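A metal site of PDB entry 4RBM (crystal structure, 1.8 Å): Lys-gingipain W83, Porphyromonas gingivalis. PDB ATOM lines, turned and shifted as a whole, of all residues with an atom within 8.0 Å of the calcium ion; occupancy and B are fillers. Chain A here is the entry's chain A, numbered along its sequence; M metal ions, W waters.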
ATOM      1  N   GLY A  84     -17.226   1.040 -12.528  1.00  0.00           N
ATOM      2  CA  GLY A  84     -16.660  -0.297 -12.485  1.00  0.00           C
ATOM      3  C   GLY A  84     -15.146  -0.239 -12.558  1.00  0.00           C
ATOM      4  O   GLY A  84     -14.557   0.805 -12.861  1.00  0.00           O
ATOM      5  N   ASP A  85     -14.527  -1.372 -12.230  1.00  0.00           N
ATOM      6  CA  ASP A  85     -13.072  -1.569 -12.331  1.00  0.00           C
ATOM      7  C   ASP A  85     -12.742  -2.031 -13.759  1.00  0.00           C
ATOM      8  O   ASP A  85     -13.617  -2.027 -14.620  1.00  0.00           O
ATOM      9  CB  ASP A  85     -12.587  -2.595 -11.273  1.00  0.00           C
ATOM     10  CG  ASP A  85     -11.140  -2.396 -10.838  1.00  0.00           C
ATOM     11  OD1 ASP A  85     -10.345  -1.840 -11.631  1.00  0.00           O
ATOM     12  OD2 ASP A  85     -10.790  -2.856  -9.735  1.00  0.00           O
ATOM     13  N   THR A  86     -11.484  -2.436 -14.023  1.00  0.00           N
ATOM     14  CA  THR A  86     -10.979  -2.797 -15.341  1.00  0.00           C
ATOM     15  C   THR A  86     -11.563  -4.114 -15.862  1.00  0.00           C
ATOM     16  O   THR A  86     -11.477  -4.344 -17.070  1.00  0.00           O
ATOM     17  CB  THR A  86      -9.471  -2.804 -15.354  1.00  0.00           C
ATOM     18  OG1 THR A  86      -9.017  -3.699 -14.343  1.00  0.00           O
ATOM     19  CG2 THR A  86      -8.903  -1.422 -15.062  1.00  0.00           C
ATOM     20  N   ASP A  87     -12.199  -4.925 -14.994  1.00  0.00           N
ATOM     21  CA  ASP A  87     -12.872  -6.170 -15.425  1.00  0.00           C
ATOM     22  C   ASP A  87     -14.162  -5.833 -16.199  1.00  0.00           C
ATOM     23  O   ASP A  87     -14.688  -6.697 -16.901  1.00  0.00           O
ATOM     24  CB  ASP A  87     -13.168  -7.114 -14.237  1.00  0.00           C
ATOM     25  CG  ASP A  87     -14.086  -6.520 -13.168  1.00  0.00           C
ATOM     26  OD1 ASP A  87     -14.111  -5.283 -13.014  1.00  0.00           O
ATOM     27  OD2 ASP A  87     -14.785  -7.304 -12.482  1.00  0.00           O
ATOM     28  N   VAL A 100      -2.216   2.116 -17.839  1.00  0.00           N
ATOM     29  CA  VAL A 100      -3.639   2.289 -18.070  1.00  0.00           C
ATOM     30  C   VAL A 100      -4.079   3.750 -17.996  1.00  0.00           C
ATOM     31  O   VAL A 100      -3.607   4.532 -17.149  1.00  0.00           O
ATOM     32  CB  VAL A 100      -4.487   1.394 -17.120  1.00  0.00           C
ATOM     33  CG1 VAL A 100      -4.459   1.895 -15.671  1.00  0.00           C
ATOM     34  CG2 VAL A 100      -5.924   1.244 -17.640  1.00  0.00           C
ATOM     35  N   ARG A 120     -13.845   7.817 -12.578  1.00  0.00           N
ATOM     36  CA  ARG A 120     -14.163   6.414 -12.472  1.00  0.00           C
ATOM     37  C   ARG A 120     -14.523   6.051 -11.043  1.00  0.00           C
ATOM     38  O   ARG A 120     -13.715   6.230 -10.153  1.00  0.00           O
ATOM     39  CB  ARG A 120     -12.978   5.567 -12.971  1.00  0.00           C
ATOM     40  CG  ARG A 120     -13.215   4.042 -12.871  1.00  0.00           C
ATOM     41  CD  ARG A 120     -11.947   3.310 -13.230  1.00  0.00           C
ATOM     42  NE  ARG A 120     -11.700   3.266 -14.675  1.00  0.00           N
ATOM     43  CZ  ARG A 120     -11.957   2.224 -15.468  1.00  0.00           C
ATOM     44  NH1 ARG A 120     -12.548   1.134 -14.963  1.00  0.00           N
ATOM     45  NH2 ARG A 120     -11.620   2.251 -16.738  1.00  0.00           N
ATOM     46  N   SER A 122     -14.565   3.270  -9.310  1.00  0.00           N
ATOM     47  CA  SER A 122     -14.045   1.912  -9.420  1.00  0.00           C
ATOM     48  C   SER A 122     -14.403   1.071  -8.199  1.00  0.00           C
ATOM     49  O   SER A 122     -14.053   1.409  -7.085  1.00  0.00           O
ATOM     50  CB  SER A 122     -12.531   1.941  -9.626  1.00  0.00           C
ATOM     51  OG  SER A 122     -12.098   0.592  -9.684  1.00  0.00           O
ATOM     52  N   ALA A 123     -15.111  -0.038  -8.439  1.00  0.00           N
ATOM     53  CA  ALA A 123     -15.525  -0.939  -7.364  1.00  0.00           C
ATOM     54  C   ALA A 123     -15.437  -2.368  -7.835  1.00  0.00           C
ATOM     55  O   ALA A 123     -15.575  -2.623  -9.032  1.00  0.00           O
ATOM     56  CB  ALA A 123     -16.958  -0.623  -6.945  1.00  0.00           C
ATOM     57  N   SER A 124     -15.196  -3.310  -6.905  1.00  0.00           N
ATOM     58  CA  SER A 124     -15.140  -4.729  -7.241  1.00  0.00           C
ATOM     59  C   SER A 124     -16.439  -5.422  -6.839  1.00  0.00           C
ATOM     60  O   SER A 124     -16.609  -6.598  -7.125  1.00  0.00           O
ATOM     61  CB  SER A 124     -13.941  -5.417  -6.595  1.00  0.00           C
ATOM     62  OG  SER A 124     -14.099  -5.552  -5.190  1.00  0.00           O
ATOM     63  N   ALA A 252      -2.687   5.795  -8.544  1.00  0.00           N
ATOM     64  CA  ALA A 252      -3.965   5.651  -9.249  1.00  0.00           C
ATOM     65  C   ALA A 252      -3.821   4.651 -10.410  1.00  0.00           C
ATOM     66  O   ALA A 252      -4.536   4.764 -11.392  1.00  0.00           O
ATOM     67  CB  ALA A 252      -4.461   7.018  -9.752  1.00  0.00           C
ATOM     68  N   GLN A 253      -2.889   3.662 -10.292  1.00  0.00           N
ATOM     69  CA  GLN A 253      -2.699   2.684 -11.368  1.00  0.00           C
ATOM     70  C   GLN A 253      -3.775   1.624 -11.176  1.00  0.00           C
ATOM     71  O   GLN A 253      -3.522   0.560 -10.604  1.00  0.00           O
ATOM     72  CB  GLN A 253      -1.264   2.131 -11.348  1.00  0.00           C
ATOM     73  CG  GLN A 253      -0.919   1.357 -12.614  1.00  0.00           C
ATOM     74  CD  GLN A 253       0.521   0.949 -12.621  1.00  0.00           C
ATOM     75  OE1 GLN A 253       0.824  -0.242 -12.469  1.00  0.00           O
ATOM     76  NE2 GLN A 253       1.442   1.911 -12.799  1.00  0.00           N
ATOM     77  N   PHE A 254      -4.984   1.937 -11.644  1.00  0.00           N
ATOM     78  CA  PHE A 254      -6.176   1.148 -11.320  1.00  0.00           C
ATOM     79  C   PHE A 254      -6.321  -0.216 -12.056  1.00  0.00           C
ATOM     80  O   PHE A 254      -7.314  -0.885 -11.787  1.00  0.00           O
ATOM     81  CB  PHE A 254      -7.466   1.976 -11.493  1.00  0.00           C
ATOM     82  CG  PHE A 254      -7.662   2.567 -12.851  1.00  0.00           C
ATOM     83  CD1 PHE A 254      -7.199   3.845 -13.150  1.00  0.00           C
ATOM     84  CD2 PHE A 254      -8.280   1.831 -13.870  1.00  0.00           C
ATOM     85  CE1 PHE A 254      -7.367   4.394 -14.438  1.00  0.00           C
ATOM     86  CE2 PHE A 254      -8.459   2.384 -15.150  1.00  0.00           C
ATOM     87  CZ  PHE A 254      -7.990   3.644 -15.429  1.00  0.00           C
ATOM     88  N   ASP A 255      -5.358  -0.640 -12.888  1.00  0.00           N
ATOM     89  CA  ASP A 255      -5.390  -1.987 -13.485  1.00  0.00           C
ATOM     90  C   ASP A 255      -4.326  -2.875 -12.787  1.00  0.00           C
ATOM     91  O   ASP A 255      -4.001  -3.935 -13.273  1.00  0.00           O
ATOM     92  CB  ASP A 255      -5.170  -1.934 -15.020  1.00  0.00           C
ATOM     93  CG  ASP A 255      -3.735  -1.716 -15.452  1.00  0.00           C
ATOM     94  OD1 ASP A 255      -2.985  -1.021 -14.712  1.00  0.00           O
ATOM     95  OD2 ASP A 255      -3.368  -2.209 -16.529  1.00  0.00           O
ATOM     96  N   TYR A 256      -3.749  -2.394 -11.686  1.00  0.00           N
ATOM     97  CA  TYR A 256      -2.742  -3.155 -10.933  1.00  0.00           C
ATOM     98  C   TYR A 256      -3.331  -4.497 -10.404  1.00  0.00           C
ATOM     99  O   TYR A 256      -4.572  -4.677 -10.314  1.00  0.00           O
ATOM    100  CB  TYR A 256      -2.192  -2.287  -9.786  1.00  0.00           C
ATOM    101  CG  TYR A 256      -1.039  -2.914  -9.042  1.00  0.00           C
ATOM    102  CD1 TYR A 256       0.165  -3.196  -9.686  1.00  0.00           C
ATOM    103  CD2 TYR A 256      -1.104  -3.119  -7.669  1.00  0.00           C
ATOM    104  CE1 TYR A 256       1.237  -3.774  -9.002  1.00  0.00           C
ATOM    105  CE2 TYR A 256      -0.037  -3.686  -6.973  1.00  0.00           C
ATOM    106  CZ  TYR A 256       1.136  -3.989  -7.637  1.00  0.00           C
ATOM    107  OH  TYR A 256       2.189  -4.542  -6.944  1.00  0.00           O
ATOM    108  N   VAL A 257      -2.439  -5.477 -10.120  1.00  0.00           N
ATOM    109  CA  VAL A 257      -2.825  -6.828  -9.656  1.00  0.00           C
ATOM    110  C   VAL A 257      -3.634  -6.751  -8.344  1.00  0.00           C
ATOM    111  O   VAL A 257      -4.474  -7.613  -8.089  1.00  0.00           O
ATOM    112  CB  VAL A 257      -1.613  -7.790  -9.535  1.00  0.00           C
ATOM    113  CG1 VAL A 257      -1.069  -8.125 -10.917  1.00  0.00           C
ATOM    114  CG2 VAL A 257      -0.512  -7.210  -8.647  1.00  0.00           C
ATOM    115  N   GLN A 258      -3.380  -5.707  -7.529  1.00  0.00           N
ATOM    116  CA  GLN A 258      -4.133  -5.446  -6.300  1.00  0.00           C
ATOM    117  C   GLN A 258      -4.898  -4.138  -6.468  1.00  0.00           C
ATOM    118  O   GLN A 258      -4.463  -3.313  -7.257  1.00  0.00           O
ATOM    119  CB  GLN A 258      -3.184  -5.312  -5.082  1.00  0.00           C
ATOM    120  CG  GLN A 258      -2.213  -6.493  -4.837  1.00  0.00           C
ATOM    121  CD  GLN A 258      -2.909  -7.794  -4.542  1.00  0.00           C
ATOM    122  OE1 GLN A 258      -3.954  -7.836  -3.876  1.00  0.00           O
ATOM    123  NE2 GLN A 258      -2.341  -8.884  -5.046  1.00  0.00           N
ATOM    124  N   PRO A 259      -5.972  -3.885  -5.702  1.00  0.00           N
ATOM    125  CA  PRO A 259      -6.609  -2.553  -5.758  1.00  0.00           C
ATOM    126  C   PRO A 259      -5.562  -1.482  -5.424  1.00  0.00           C
ATOM    127  O   PRO A 259      -4.807  -1.641  -4.446  1.00  0.00           O
ATOM    128  CB  PRO A 259      -7.670  -2.646  -4.646  1.00  0.00           C
ATOM    129  CG  PRO A 259      -8.018  -4.105  -4.592  1.00  0.00           C
ATOM    130  CD  PRO A 259      -6.658  -4.751  -4.713  1.00  0.00           C
ATOM    131  N   CYS A 260      -5.463  -0.436  -6.279  1.00  0.00           N
ATOM    132  CA  CYS A 260      -4.474   0.599  -6.040  1.00  0.00           C
ATOM    133  C   CYS A 260      -4.915   1.482  -4.881  1.00  0.00           C
ATOM    134  O   CYS A 260      -6.082   1.434  -4.469  1.00  0.00           O
ATOM    135  CB  CYS A 260      -4.194   1.411  -7.294  1.00  0.00           C
ATOM    136  SG  CYS A 260      -5.591   2.426  -7.832  1.00  0.00           S
ATOM    137  N   GLU A 263      -8.048   3.480  -5.442  1.00  0.00           N
ATOM    138  CA  GLU A 263      -9.244   2.633  -5.375  1.00  0.00           C
ATOM    139  C   GLU A 263      -9.579   2.352  -3.946  1.00  0.00           C
ATOM    140  O   GLU A 263     -10.744   2.515  -3.567  1.00  0.00           O
ATOM    141  CB  GLU A 263      -9.070   1.322  -6.173  1.00  0.00           C
ATOM    142  CG  GLU A 263      -9.152   1.549  -7.679  1.00  0.00           C
ATOM    143  CD  GLU A 263      -8.795   0.309  -8.484  1.00  0.00           C
ATOM    144  OE1 GLU A 263      -7.786  -0.372  -8.178  1.00  0.00           O
ATOM    145  OE2 GLU A 263      -9.586  -0.017  -9.394  1.00  0.00           O
ATOM    146  N   ARG A 267     -12.959   3.240  -1.973  1.00  0.00           N
ATOM    147  CA  ARG A 267     -13.831   2.091  -1.685  1.00  0.00           C
ATOM    148  C   ARG A 267     -14.084   1.834  -0.199  1.00  0.00           C
ATOM    149  O   ARG A 267     -15.088   1.181   0.126  1.00  0.00           O
ATOM    150  CB  ARG A 267     -13.227   0.818  -2.268  1.00  0.00           C
ATOM    151  CG  ARG A 267     -13.270   0.752  -3.778  1.00  0.00           C
ATOM    152  CD  ARG A 267     -12.409  -0.405  -4.241  1.00  0.00           C
ATOM    153  NE  ARG A 267     -12.444  -0.524  -5.704  1.00  0.00           N
ATOM    154  CZ  ARG A 267     -11.956  -1.557  -6.368  1.00  0.00           C
ATOM    155  NH1 ARG A 267     -11.417  -2.589  -5.719  1.00  0.00           N
ATOM    156  NH2 ARG A 267     -12.048  -1.605  -7.691  1.00  0.00           N
ATOM    157  N   LEU A 360     -10.572   9.099  -9.280  1.00  0.00           N
ATOM    158  CA  LEU A 360     -11.226   7.865  -8.809  1.00  0.00           C
ATOM    159  C   LEU A 360     -12.268   8.324  -7.778  1.00  0.00           C
ATOM    160  O   LEU A 360     -11.997   9.254  -7.031  1.00  0.00           O
ATOM    161  CB  LEU A 360     -10.211   6.871  -8.242  1.00  0.00           C
ATOM    162  CG  LEU A 360      -9.312   6.172  -9.304  1.00  0.00           C
ATOM    163  CD1 LEU A 360      -8.090   5.529  -8.623  1.00  0.00           C
ATOM    164  CD2 LEU A 360     -10.098   5.014 -10.073  1.00  0.00           C
HETATM  165 CA    CA M   1      -8.387  -2.046 -10.070  1.00  0.00          CA
HETATM  166  O   HOH W   1      -8.360  -3.787  -8.272  1.00  0.00           O
HETATM  167  O   HOH W   2      -5.970  -2.419  -9.511  1.00  0.00           O
HETATM  168  O   HOH W   3      -8.001  -3.957 -11.638  1.00  0.00           O
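The backbone carbonyl oxygen of Asp 85 lies within hydrogen-bond range of the guanidinium group of Arg 120 (3.4 Å).
OE2 of Glu 263 lies close to OG of Ser 122.
The side-chain carboxylate (OE2) of Glu 263 lies close to the guanidinium group (NH2) of Arg 267.
The guanidinium group (NH2) of Arg 267 lies close to the side-chain carboxylate (OD2) of Asp 85 (2.7 Å).
The side-chain sulfur (SG) of Cys 260 lies within hydrogen-bond range of the backbone NH (N) of Glu 263 (3.6 Å).
Of the 21 residues printed, 3 come within 4 Å of the calcium ion.
Along chain A the residues within 4 Å of the calcium ion span positions 85 to 263.
O of Phe 254 binds the calcium ion (2.3 Å).
OE2 of Glu 263 binds the calcium ion, at 2.5 Å.
The calcium ion is bound by water W3, at 2.5 Å.
Water W1 is bound to the calcium ion (2.5 Å).
Water W2 is bound to the calcium ion, 2.5 Å away.
OD1 of Asp 85 binds the calcium ion (2.5 Å).
The calcium ion is bound by the side-chain carboxylate (OD2) of Asp 85.
OE1 of Glu 263 binds the calcium ion.
The calcium ion has eight donor atoms within binding distance.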
